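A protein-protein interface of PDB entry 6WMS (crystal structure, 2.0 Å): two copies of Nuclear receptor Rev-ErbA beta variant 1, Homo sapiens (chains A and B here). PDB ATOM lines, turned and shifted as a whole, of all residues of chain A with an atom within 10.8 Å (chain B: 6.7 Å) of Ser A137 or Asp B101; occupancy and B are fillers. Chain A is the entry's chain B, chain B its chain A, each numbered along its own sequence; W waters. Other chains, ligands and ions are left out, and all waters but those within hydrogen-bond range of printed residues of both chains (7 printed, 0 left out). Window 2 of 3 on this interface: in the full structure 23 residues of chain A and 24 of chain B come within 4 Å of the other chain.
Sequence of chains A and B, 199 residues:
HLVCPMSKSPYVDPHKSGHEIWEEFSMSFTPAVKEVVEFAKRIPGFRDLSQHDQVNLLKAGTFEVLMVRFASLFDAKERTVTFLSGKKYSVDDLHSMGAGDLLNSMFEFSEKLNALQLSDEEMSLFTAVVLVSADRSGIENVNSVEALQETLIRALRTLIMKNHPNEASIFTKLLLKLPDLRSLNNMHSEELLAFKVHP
No position is printed for both chains.
Hydrophobic or aromatic side chains of chain B within 4 Å of the printed part of chain A: Met B187.
Of the 25 printed residues of chain A, 4 touch a printed residue of chain B.
Among the printed residues, no Asp or Glu carboxylate lies within 4 Å of a Lys or Arg side-chain nitrogen of the other chain.
Among the printed residues, pairs that only touch across the chains: Asp A135 with Ser B183 (3.6 Å), Ser A137 with Asp B101 (3.5 Å), Ser A137 with Ser B105 (3.999 Å) and Val A142 with Glu B108 (3.6 Å).
The side-chain sulfur (SD) of Met B187 is in hydrogen-bond range of the side-chain hydroxyl (OG) of Ser A137 (3.2 Å).
NH1 of Arg A182 sits at hydrogen-bond distance from OG of Ser B183 (2.8 Å).
Water W1 lies within hydrogen-bond range of the side-chain sulfur of Met B187, the side-chain hydroxyl of Ser B105, the side-chain hydroxyl of Ser A137, the backbone carbonyl oxygen of Asp B101 and the backbone NH of Leu B102.
Water W2 bridges the backbone carbonyl oxygen (O) of Arg A136 (2.6 Å) and the side-chain carboxylate (OE2) of Glu B108 (3.0 Å).
Water W6 lies within hydrogen-bond range of the side-chain hydroxyl of Ser B105 (2.8 Å), the backbone NH of Ser A137 (3.2 Å) and the backbone carbonyl oxygen of Arg A136 (3.3 Å).
Water W3 bridges the side-chain amide oxygen of Asn A186 (2.8 Å) and the side-chain hydroxyl of Ser B183 (3.0 Å).
Water W4 lies within hydrogen-bond range of O of Ser A137 (2.9 Å), OG of Ser B105 (2.9 Å) and O of Asp B101 (3.0 Å).
Water W5 lies within hydrogen-bond range of the side-chain hydroxyl of Ser A137 (2.9 Å) and the side-chain carboxylate of Asp B101 (2.9 Å).
OE2 of Glu A64 lies within salt-bridge range of NE of Arg A182.
The backbone NH (N) of Ser A137 is in hydrogen-bond range of the side-chain carboxylate (OD1) of Asp A135, at 3.1 Å.
The backbone carbonyl oxygen (O) of Ser A133 lies within hydrogen-bond range of the guanidinium group (NH2) of Arg A182 (2.7 Å).
O of Asp B101 sits at hydrogen-bond distance from OG of Ser B105.
The backbone carbonyl oxygen (O) of Arg A182 lies close to the side-chain amide oxygen (OD1) of Asn A186 (3.4 Å).
Of the printed residues of chain B, Ser A137 touches Asp B101, Ser B105 and Met B187.
Of chain A, only Ser A137 comes within 4 Å of Asp B101.
Gly B100 touches none of the printed residues of chain A.
No residue of chain A comes within 4 Å of Leu B102.
Printed residues of chain B within 4 Å of Asp A135: Ser B183.
Of the printed residues of chain A, Ser B105 touches Ser A137 (3.999 Å).
Printed residues of chain A within 4 Å of Met B187: Ser A137.
Asn A56 touches none of the printed residues of chain B.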
ATOM      1  N   HIS A  52      14.243  21.250 -34.111  1.00  0.00           N
ATOM      2  CA  HIS A  52      13.416  21.147 -32.912  1.00  0.00           C
ATOM      3  C   HIS A  52      12.407  22.290 -32.848  1.00  0.00           C
ATOM      4  O   HIS A  52      11.221  22.078 -32.575  1.00  0.00           O
ATOM      5  CB  HIS A  52      14.291  21.145 -31.661  1.00  0.00           C
ATOM      6  CG  HIS A  52      13.514  21.177 -30.381  1.00  0.00           C
ATOM      7  ND1 HIS A  52      13.169  22.352 -29.747  1.00  0.00           N
ATOM      8  CD2 HIS A  52      13.019  20.176 -29.612  1.00  0.00           C
ATOM      9  CE1 HIS A  52      12.500  22.075 -28.641  1.00  0.00           C
ATOM     10  NE2 HIS A  52      12.388  20.761 -28.540  1.00  0.00           N
ATOM     11  N   ASP A  53      12.863  23.513 -33.095  1.00  0.00           N
ATOM     12  CA  ASP A  53      11.960  24.645 -32.950  1.00  0.00           C
ATOM     13  C   ASP A  53      10.936  24.673 -34.083  1.00  0.00           C
ATOM     14  O   ASP A  53       9.769  25.023 -33.861  1.00  0.00           O
ATOM     15  CB  ASP A  53      12.763  25.944 -32.872  1.00  0.00           C
ATOM     16  CG  ASP A  53      13.489  26.118 -31.527  1.00  0.00           C
ATOM     17  OD1 ASP A  53      13.153  25.418 -30.548  1.00  0.00           O
ATOM     18  OD2 ASP A  53      14.388  26.979 -31.441  1.00  0.00           O
ATOM     19  N   VAL A  55       9.546  22.058 -35.468  1.00  0.00           N
ATOM     20  CA  VAL A  55       8.501  21.083 -35.163  1.00  0.00           C
ATOM     21  C   VAL A  55       7.615  21.584 -34.036  1.00  0.00           C
ATOM     22  O   VAL A  55       6.396  21.367 -34.041  1.00  0.00           O
ATOM     23  CB  VAL A  55       9.124  19.715 -34.823  1.00  0.00           C
ATOM     24  CG1 VAL A  55       8.059  18.751 -34.273  1.00  0.00           C
ATOM     25  CG2 VAL A  55       9.812  19.131 -36.038  1.00  0.00           C
ATOM     26  N   ASN A  56       8.206  22.257 -33.049  1.00  0.00           N
ATOM     27  CA  ASN A  56       7.412  22.773 -31.940  1.00  0.00           C
ATOM     28  C   ASN A  56       6.466  23.871 -32.394  1.00  0.00           C
ATOM     29  O   ASN A  56       5.323  23.938 -31.929  1.00  0.00           O
ATOM     30  CB  ASN A  56       8.315  23.291 -30.831  1.00  0.00           C
ATOM     31  CG  ASN A  56       8.574  22.249 -29.777  1.00  0.00           C
ATOM     32  OD1 ASN A  56       9.720  21.944 -29.467  1.00  0.00           O
ATOM     33  ND2 ASN A  56       7.505  21.674 -29.236  1.00  0.00           N
ATOM     34  N   LEU A  57       6.925  24.750 -33.287  1.00  0.00           N
ATOM     35  CA  LEU A  57       6.044  25.802 -33.779  1.00  0.00           C
ATOM     36  C   LEU A  57       4.887  25.197 -34.564  1.00  0.00           C
ATOM     37  O   LEU A  57       3.729  25.596 -34.400  1.00  0.00           O
ATOM     38  CB  LEU A  57       6.834  26.792 -34.636  1.00  0.00           C
ATOM     39  CG  LEU A  57       7.651  27.895 -33.949  1.00  0.00           C
ATOM     40  CD1 LEU A  57       8.134  28.890 -35.007  1.00  0.00           C
ATOM     41  CD2 LEU A  57       6.883  28.630 -32.807  1.00  0.00           C
ATOM     42  N   LEU A  58       5.183  24.212 -35.411  1.00  0.00           N
ATOM     43  CA  LEU A  58       4.124  23.534 -36.154  1.00  0.00           C
ATOM     44  C   LEU A  58       3.211  22.745 -35.224  1.00  0.00           C
ATOM     45  O   LEU A  58       1.995  22.705 -35.429  1.00  0.00           O
ATOM     46  CB  LEU A  58       4.741  22.610 -37.208  1.00  0.00           C
ATOM     47  CG  LEU A  58       5.165  23.418 -38.427  1.00  0.00           C
ATOM     48  CD1 LEU A  58       6.215  22.681 -39.266  1.00  0.00           C
ATOM     49  CD2 LEU A  58       3.906  23.733 -39.217  1.00  0.00           C
ATOM     50  N   LYS A  59       3.786  22.081 -34.219  1.00  0.00           N
ATOM     51  CA  LYS A  59       2.978  21.355 -33.249  1.00  0.00           C
ATOM     52  C   LYS A  59       1.980  22.289 -32.584  1.00  0.00           C
ATOM     53  O   LYS A  59       0.788  21.977 -32.478  1.00  0.00           O
ATOM     54  CB  LYS A  59       3.879  20.714 -32.192  1.00  0.00           C
ATOM     55  CG  LYS A  59       4.091  19.224 -32.360  1.00  0.00           C
ATOM     56  CD  LYS A  59       4.077  18.507 -31.008  1.00  0.00           C
ATOM     57  CE  LYS A  59       5.328  18.808 -30.198  1.00  0.00           C
ATOM     58  NZ  LYS A  59       5.450  17.880 -29.030  1.00  0.00           N
ATOM     59  N   ALA A  60       2.452  23.455 -32.154  1.00  0.00           N
ATOM     60  CA  ALA A  60       1.600  24.385 -31.427  1.00  0.00           C
ATOM     61  C   ALA A  60       0.730  25.234 -32.350  1.00  0.00           C
ATOM     62  O   ALA A  60      -0.333  25.704 -31.921  1.00  0.00           O
ATOM     63  CB  ALA A  60       2.470  25.281 -30.539  1.00  0.00           C
ATOM     64  N   GLY A  61       1.143  25.452 -33.602  1.00  0.00           N
ATOM     65  CA  GLY A  61       0.462  26.434 -34.431  1.00  0.00           C
ATOM     66  C   GLY A  61      -0.340  25.919 -35.614  1.00  0.00           C
ATOM     67  O   GLY A  61      -1.012  26.700 -36.304  1.00  0.00           O
ATOM     68  N   GLU A  64      -4.041  26.722 -35.564  1.00  0.00           N
ATOM     69  CA  GLU A  64      -4.378  28.127 -35.762  1.00  0.00           C
ATOM     70  C   GLU A  64      -4.205  28.534 -37.218  1.00  0.00           C
ATOM     71  O   GLU A  64      -4.983  29.352 -37.727  1.00  0.00           O
ATOM     72  CB  GLU A  64      -3.554  29.008 -34.823  1.00  0.00           C
ATOM     73  CG  GLU A  64      -3.848  28.725 -33.331  1.00  0.00           C
ATOM     74  CD  GLU A  64      -2.917  29.465 -32.364  1.00  0.00           C
ATOM     75  OE1 GLU A  64      -2.662  30.671 -32.578  1.00  0.00           O
ATOM     76  OE2 GLU A  64      -2.453  28.844 -31.384  1.00  0.00           O
ATOM     77  N   LEU A 131       1.524  31.409 -37.769  1.00  0.00           N
ATOM     78  CA  LEU A 131       2.369  30.249 -37.482  1.00  0.00           C
ATOM     79  C   LEU A 131       3.575  30.623 -36.620  1.00  0.00           C
ATOM     80  O   LEU A 131       3.882  29.946 -35.626  1.00  0.00           O
ATOM     81  CB  LEU A 131       2.842  29.596 -38.784  1.00  0.00           C
ATOM     82  CG  LEU A 131       3.856  28.483 -38.481  1.00  0.00           C
ATOM     83  CD1 LEU A 131       3.258  27.435 -37.530  1.00  0.00           C
ATOM     84  CD2 LEU A 131       4.302  27.847 -39.763  1.00  0.00           C
ATOM     85  N   VAL A 132       4.300  31.677 -36.996  1.00  0.00           N
ATOM     86  CA  VAL A 132       5.511  31.991 -36.243  1.00  0.00           C
ATOM     87  C   VAL A 132       5.211  32.632 -34.893  1.00  0.00           C
ATOM     88  O   VAL A 132       6.111  32.721 -34.050  1.00  0.00           O
ATOM     89  CB  VAL A 132       6.459  32.867 -37.088  1.00  0.00           C
ATOM     90  CG1 VAL A 132       6.859  32.110 -38.374  1.00  0.00           C
ATOM     91  CG2 VAL A 132       5.799  34.199 -37.404  1.00  0.00           C
ATOM     92  N   SER A 133       3.963  33.027 -34.633  1.00  0.00           N
ATOM     93  CA  SER A 133       3.562  33.527 -33.318  1.00  0.00           C
ATOM     94  C   SER A 133       3.037  32.428 -32.392  1.00  0.00           C
ATOM     95  O   SER A 133       2.533  32.738 -31.302  1.00  0.00           O
ATOM     96  CB  SER A 133       2.496  34.626 -33.468  1.00  0.00           C
ATOM     97  OG  SER A 133       2.985  35.720 -34.227  1.00  0.00           O
ATOM     98  N   ALA A 134       3.148  31.161 -32.790  1.00  0.00           N
ATOM     99  CA  ALA A 134       2.658  30.061 -31.962  1.00  0.00           C
ATOM    100  C   ALA A 134       3.313  30.062 -30.574  1.00  0.00           C
ATOM    101  O   ALA A 134       4.390  30.624 -30.361  1.00  0.00           O
ATOM    102  CB  ALA A 134       2.907  28.716 -32.645  1.00  0.00           C
ATOM    103  N   ASP A 135       2.606  29.456 -29.619  1.00  0.00           N
ATOM    104  CA  ASP A 135       3.078  29.264 -28.249  1.00  0.00           C
ATOM    105  C   ASP A 135       4.545  28.849 -28.248  1.00  0.00           C
ATOM    106  O   ASP A 135       4.932  27.909 -28.939  1.00  0.00           O
ATOM    107  CB  ASP A 135       2.210  28.183 -27.573  1.00  0.00           C
ATOM    108  CG  ASP A 135       2.573  27.937 -26.108  1.00  0.00           C
ATOM    109  OD1 ASP A 135       3.383  28.685 -25.524  1.00  0.00           O
ATOM    110  OD2 ASP A 135       2.014  26.976 -25.530  1.00  0.00           O
ATOM    111  N   ARG A 136       5.364  29.572 -27.495  1.00  0.00           N
ATOM    112  CA  ARG A 136       6.799  29.320 -27.498  1.00  0.00           C
ATOM    113  C   ARG A 136       7.251  28.475 -26.317  1.00  0.00           C
ATOM    114  O   ARG A 136       8.444  28.460 -25.990  1.00  0.00           O
ATOM    115  CB  ARG A 136       7.557  30.639 -27.534  1.00  0.00           C
ATOM    116  CG  ARG A 136       7.403  31.323 -28.882  1.00  0.00           C
ATOM    117  CD  ARG A 136       8.273  32.552 -29.007  1.00  0.00           C
ATOM    118  NE  ARG A 136       7.898  33.565 -28.033  1.00  0.00           N
ATOM    119  CZ  ARG A 136       6.825  34.337 -28.154  1.00  0.00           C
ATOM    120  NH1 ARG A 136       6.028  34.195 -29.211  1.00  0.00           N
ATOM    121  NH2 ARG A 136       6.550  35.245 -27.223  1.00  0.00           N
ATOM    122  N   SER A 137       6.330  27.745 -25.695  1.00  0.00           N
ATOM    123  CA  SER A 137       6.660  27.049 -24.459  1.00  0.00           C
ATOM    124  C   SER A 137       7.708  25.956 -24.696  1.00  0.00           C
ATOM    125  O   SER A 137       8.621  25.780 -23.882  1.00  0.00           O
ATOM    126  CB  SER A 137       5.380  26.492 -23.835  1.00  0.00           C
ATOM    127  OG  SER A 137       5.653  25.465 -22.902  1.00  0.00           O
ATOM    128  N   GLY A 138       7.633  25.243 -25.822  1.00  0.00           N
ATOM    129  CA  GLY A 138       8.683  24.267 -26.098  1.00  0.00           C
ATOM    130  C   GLY A 138      10.023  24.842 -26.548  1.00  0.00           C
ATOM    131  O   GLY A 138      11.055  24.178 -26.388  1.00  0.00           O
ATOM    132  N   ILE A 139      10.038  26.080 -27.047  1.00  0.00           N
ATOM    133  CA  ILE A 139      11.059  26.518 -27.995  1.00  0.00           C
ATOM    134  C   ILE A 139      12.431  26.637 -27.338  1.00  0.00           C
ATOM    135  O   ILE A 139      12.570  27.112 -26.202  1.00  0.00           O
ATOM    136  CB  ILE A 139      10.624  27.846 -28.640  1.00  0.00           C
ATOM    137  CG1 ILE A 139       9.352  27.619 -29.466  1.00  0.00           C
ATOM    138  CG2 ILE A 139      11.739  28.430 -29.503  1.00  0.00           C
ATOM    139  CD1 ILE A 139       9.600  26.969 -30.814  1.00  0.00           C
ATOM    140  N   GLU A 140      13.463  26.217 -28.068  1.00  0.00           N
ATOM    141  CA  GLU A 140      14.825  26.220 -27.541  1.00  0.00           C
ATOM    142  C   GLU A 140      15.511  27.560 -27.771  1.00  0.00           C
ATOM    143  O   GLU A 140      16.143  28.108 -26.865  1.00  0.00           O
ATOM    144  CB  GLU A 140      15.633  25.089 -28.186  1.00  0.00           C
ATOM    145  CG  GLU A 140      15.715  23.836 -27.331  1.00  0.00           C
ATOM    146  CD  GLU A 140      16.145  22.610 -28.120  1.00  0.00           C
ATOM    147  OE1 GLU A 140      15.743  21.495 -27.729  1.00  0.00           O
ATOM    148  OE2 GLU A 140      16.876  22.759 -29.126  1.00  0.00           O
ATOM    149  N   ASN A 141      15.391  28.099 -28.979  1.00  0.00           N
ATOM    150  CA  ASN A 141      16.000  29.373 -29.326  1.00  0.00           C
ATOM    151  C   ASN A 141      14.845  30.348 -29.542  1.00  0.00           C
ATOM    152  O   ASN A 141      14.379  30.551 -30.667  1.00  0.00           O
ATOM    153  CB  ASN A 141      16.903  29.225 -30.576  1.00  0.00           C
ATOM    154  CG  ASN A 141      17.522  30.555 -31.028  1.00  0.00           C
ATOM    155  OD1 ASN A 141      18.134  30.620 -32.096  1.00  0.00           O
ATOM    156  ND2 ASN A 141      17.396  31.600 -30.208  1.00  0.00           N
ATOM    157  N   VAL A 142      14.377  30.948 -28.441  1.00  0.00           N
ATOM    158  CA  VAL A 142      13.248  31.874 -28.516  1.00  0.00           C
ATOM    159  C   VAL A 142      13.627  33.127 -29.293  1.00  0.00           C
ATOM    160  O   VAL A 142      12.786  33.715 -29.982  1.00  0.00           O
ATOM    161  CB  VAL A 142      12.731  32.214 -27.101  1.00  0.00           C
ATOM    162  CG1 VAL A 142      12.173  30.971 -26.423  1.00  0.00           C
ATOM    163  CG2 VAL A 142      13.846  32.811 -26.258  1.00  0.00           C
ATOM    164  N   VAL A 145      13.011  32.693 -33.079  1.00  0.00           N
ATOM    165  CA  VAL A 145      11.590  32.756 -33.404  1.00  0.00           C
ATOM    166  C   VAL A 145      11.080  34.181 -33.259  1.00  0.00           C
ATOM    167  O   VAL A 145      10.339  34.676 -34.112  1.00  0.00           O
ATOM    168  CB  VAL A 145      10.800  31.770 -32.527  1.00  0.00           C
ATOM    169  CG1 VAL A 145       9.294  31.867 -32.821  1.00  0.00           C
ATOM    170  CG2 VAL A 145      11.334  30.338 -32.740  1.00  0.00           C
ATOM    171  N   ARG A 182      -5.582  31.949 -30.235  1.00  0.00           N
ATOM    172  CA  ARG A 182      -4.942  31.147 -29.204  1.00  0.00           C
ATOM    173  C   ARG A 182      -5.984  30.538 -28.280  1.00  0.00           C
ATOM    174  O   ARG A 182      -5.837  29.394 -27.842  1.00  0.00           O
ATOM    175  CB  ARG A 182      -3.933  31.989 -28.413  1.00  0.00           C
ATOM    176  CG  ARG A 182      -3.067  31.170 -27.465  1.00  0.00           C
ATOM    177  CD  ARG A 182      -2.111  30.263 -28.262  1.00  0.00           C
ATOM    178  NE  ARG A 182      -1.566  30.959 -29.420  1.00  0.00           N
ATOM    179  CZ  ARG A 182      -0.449  31.671 -29.397  1.00  0.00           C
ATOM    180  NH1 ARG A 182       0.241  31.770 -28.262  1.00  0.00           N
ATOM    181  NH2 ARG A 182      -0.025  32.278 -30.510  1.00  0.00           N
ATOM    182  N   ASN A 186      -6.674  26.647 -27.559  1.00  0.00           N
ATOM    183  CA  ASN A 186      -6.743  26.090 -26.208  1.00  0.00           C
ATOM    184  C   ASN A 186      -7.996  25.242 -26.024  1.00  0.00           C
ATOM    185  O   ASN A 186      -7.934  24.117 -25.519  1.00  0.00           O
ATOM    186  CB  ASN A 186      -6.753  27.215 -25.174  1.00  0.00           C
ATOM    187  CG  ASN A 186      -5.410  27.931 -25.045  1.00  0.00           C
ATOM    188  OD1 ASN A 186      -4.370  27.436 -25.469  1.00  0.00           O
ATOM    189  ND2 ASN A 186      -5.446  29.124 -24.453  1.00  0.00           N
ATOM    190  N   HIS B  95      13.399  25.459 -10.012  1.00  0.00           N
ATOM    191  CA  HIS B  95      13.384  24.312 -10.905  1.00  0.00           C
ATOM    192  C   HIS B  95      13.625  23.026 -10.123  1.00  0.00           C
ATOM    193  O   HIS B  95      12.977  22.011 -10.380  1.00  0.00           O
ATOM    194  CB  HIS B  95      14.406  24.492 -12.036  1.00  0.00           C
ATOM    195  CG  HIS B  95      13.852  25.226 -13.226  1.00  0.00           C
ATOM    196  ND1 HIS B  95      14.569  26.166 -13.938  1.00  0.00           N
ATOM    197  CD2 HIS B  95      12.629  25.175 -13.805  1.00  0.00           C
ATOM    198  CE1 HIS B  95      13.814  26.647 -14.913  1.00  0.00           C
ATOM    199  NE2 HIS B  95      12.630  26.066 -14.851  1.00  0.00           N
ATOM    200  N   ALA B  99       9.580  23.529 -10.637  1.00  0.00           N
ATOM    201  CA  ALA B  99       9.226  24.470 -11.692  1.00  0.00           C
ATOM    202  C   ALA B  99       9.825  24.014 -13.016  1.00  0.00           C
ATOM    203  O   ALA B  99      10.782  23.233 -13.062  1.00  0.00           O
ATOM    204  CB  ALA B  99       9.708  25.887 -11.365  1.00  0.00           C
ATOM    205  N   GLY B 100       9.263  24.520 -14.107  1.00  0.00           N
ATOM    206  CA  GLY B 100       9.684  24.044 -15.412  1.00  0.00           C
ATOM    207  C   GLY B 100       9.572  25.083 -16.506  1.00  0.00           C
ATOM    208  O   GLY B 100       9.964  26.237 -16.326  1.00  0.00           O
ATOM    209  N   ASP B 101       9.037  24.671 -17.657  1.00  0.00           N
ATOM    210  CA  ASP B 101       8.986  25.567 -18.803  1.00  0.00           C
ATOM    211  C   ASP B 101       8.086  26.770 -18.544  1.00  0.00           C
ATOM    212  O   ASP B 101       8.323  27.847 -19.102  1.00  0.00           O
ATOM    213  CB  ASP B 101       8.499  24.811 -20.031  1.00  0.00           C
ATOM    214  CG  ASP B 101       9.588  23.932 -20.651  1.00  0.00           C
ATOM    215  OD1 ASP B 101      10.757  23.968 -20.183  1.00  0.00           O
ATOM    216  OD2 ASP B 101       9.261  23.193 -21.604  1.00  0.00           O
ATOM    217  N   LEU B 102       7.029  26.602 -17.739  1.00  0.00           N
ATOM    218  CA  LEU B 102       6.136  27.727 -17.483  1.00  0.00           C
ATOM    219  C   LEU B 102       6.891  28.866 -16.809  1.00  0.00           C
ATOM    220  O   LEU B 102       6.832  30.009 -17.261  1.00  0.00           O
ATOM    221  CB  LEU B 102       4.937  27.298 -16.636  1.00  0.00           C
ATOM    222  CG  LEU B 102       3.973  28.467 -16.350  1.00  0.00           C
ATOM    223  CD1 LEU B 102       3.575  29.244 -17.613  1.00  0.00           C
ATOM    224  CD2 LEU B 102       2.726  27.938 -15.632  1.00  0.00           C
ATOM    225  N   LEU B 103       7.617  28.567 -15.726  1.00  0.00           N
ATOM    226  CA  LEU B 103       8.442  29.593 -15.087  1.00  0.00           C
ATOM    227  C   LEU B 103       9.361  30.276 -16.095  1.00  0.00           C
ATOM    228  O   LEU B 103       9.482  31.505 -16.102  1.00  0.00           O
ATOM    229  CB  LEU B 103       9.259  28.977 -13.953  1.00  0.00           C
ATOM    230  CG  LEU B 103      10.193  29.974 -13.250  1.00  0.00           C
ATOM    231  CD1 LEU B 103       9.445  31.171 -12.665  1.00  0.00           C
ATOM    232  CD2 LEU B 103      11.036  29.263 -12.177  1.00  0.00           C
ATOM    233  N   ASN B 104      10.029  29.487 -16.954  1.00  0.00           N
ATOM    234  CA  ASN B 104      10.926  30.069 -17.952  1.00  0.00           C
ATOM    235  C   ASN B 104      10.176  31.025 -18.867  1.00  0.00           C
ATOM    236  O   ASN B 104      10.678  32.110 -19.195  1.00  0.00           O
ATOM    237  CB  ASN B 104      11.577  28.978 -18.813  1.00  0.00           C
ATOM    238  CG  ASN B 104      12.644  28.177 -18.073  1.00  0.00           C
ATOM    239  OD1 ASN B 104      13.147  28.594 -17.028  1.00  0.00           O
ATOM    240  ND2 ASN B 104      13.004  27.018 -18.635  1.00  0.00           N
ATOM    241  N   SER B 105       8.987  30.610 -19.322  1.00  0.00           N
ATOM    242  CA  SER B 105       8.155  31.459 -20.166  1.00  0.00           C
ATOM    243  C   SER B 105       7.742  32.742 -19.452  1.00  0.00           C
ATOM    244  O   SER B 105       7.600  33.785 -20.095  1.00  0.00           O
ATOM    245  CB  SER B 105       6.917  30.691 -20.627  1.00  0.00           C
ATOM    246  OG  SER B 105       7.278  29.555 -21.405  1.00  0.00           O
ATOM    247  N   MET B 106       7.547  32.692 -18.125  1.00  0.00           N
ATOM    248  CA  MET B 106       7.159  33.903 -17.401  1.00  0.00           C
ATOM    249  C   MET B 106       8.327  34.874 -17.255  1.00  0.00           C
ATOM    250  O   MET B 106       8.127  36.095 -17.274  1.00  0.00           O
ATOM    251  CB  MET B 106       6.599  33.550 -16.025  1.00  0.00           C
ATOM    252  CG  MET B 106       5.175  33.044 -16.065  1.00  0.00           C
ATOM    253  SD  MET B 106       4.648  32.541 -14.415  1.00  0.00           S
ATOM    254  CE  MET B 106       2.975  32.005 -14.800  1.00  0.00           C
ATOM    255  N   GLU B 108      10.642  35.171 -19.592  1.00  0.00           N
ATOM    256  CA  GLU B 108      10.734  35.764 -20.928  1.00  0.00           C
ATOM    257  C   GLU B 108       9.677  36.844 -21.130  1.00  0.00           C
ATOM    258  O   GLU B 108       9.975  37.920 -21.655  1.00  0.00           O
ATOM    259  CB  GLU B 108      10.607  34.669 -21.995  1.00  0.00           C
ATOM    260  CG  GLU B 108      11.754  33.632 -21.905  1.00  0.00           C
ATOM    261  CD  GLU B 108      11.492  32.330 -22.654  1.00  0.00           C
ATOM    262  OE1 GLU B 108      12.469  31.573 -22.871  1.00  0.00           O
ATOM    263  OE2 GLU B 108      10.323  32.048 -23.010  1.00  0.00           O
ATOM    264  N   SER B 183      -1.330  32.027 -23.668  1.00  0.00           N
ATOM    265  CA  SER B 183      -0.644  30.746 -23.529  1.00  0.00           C
ATOM    266  C   SER B 183      -0.189  30.519 -22.096  1.00  0.00           C
ATOM    267  O   SER B 183      -0.332  29.411 -21.561  1.00  0.00           O
ATOM    268  CB  SER B 183       0.550  30.690 -24.479  1.00  0.00           C
ATOM    269  OG  SER B 183       0.079  30.506 -25.801  1.00  0.00           O
ATOM    270  N   LEU B 184       0.367  31.554 -21.464  1.00  0.00           N
ATOM    271  CA  LEU B 184       0.753  31.447 -20.065  1.00  0.00           C
ATOM    272  C   LEU B 184      -0.426  31.019 -19.222  1.00  0.00           C
ATOM    273  O   LEU B 184      -0.284  30.171 -18.343  1.00  0.00           O
ATOM    274  CB  LEU B 184       1.274  32.782 -19.551  1.00  0.00           C
ATOM    275  CG  LEU B 184       2.575  33.277 -20.167  1.00  0.00           C
ATOM    276  CD1 LEU B 184       2.853  34.642 -19.587  1.00  0.00           C
ATOM    277  CD2 LEU B 184       3.702  32.290 -19.852  1.00  0.00           C
ATOM    278  N   MET B 187      -1.315  27.198 -19.839  1.00  0.00           N
ATOM    279  CA  MET B 187      -0.360  26.309 -19.177  1.00  0.00           C
ATOM    280  C   MET B 187      -0.492  26.384 -17.661  1.00  0.00           C
ATOM    281  O   MET B 187      -0.492  25.356 -16.953  1.00  0.00           O
ATOM    282  CB  MET B 187       1.053  26.703 -19.597  1.00  0.00           C
ATOM    283  CG  MET B 187       1.694  25.774 -20.588  1.00  0.00           C
ATOM    284  SD  MET B 187       3.312  26.441 -20.997  1.00  0.00           S
ATOM    285  CE  MET B 187       2.862  28.124 -21.499  1.00  0.00           C
HETATM  286  O   HOH W   1       5.692  27.380 -20.812  1.00  0.00           O
HETATM  287  O   HOH W   2      10.050  29.298 -24.128  1.00  0.00           O
HETATM  288  O   HOH W   3      -1.600  28.005 -25.823  1.00  0.00           O
HETATM  289  O   HOH W   4       9.482  27.663 -21.917  1.00  0.00           O
HETATM  290  O   HOH W   5       6.560  22.706 -22.645  1.00  0.00           O
HETATM  291  O   HOH W   6       6.662  30.434 -24.017  1.00  0.00           O
HETATM  292  O   HOH W   7      -0.516  26.852 -23.312  1.00  0.00           O
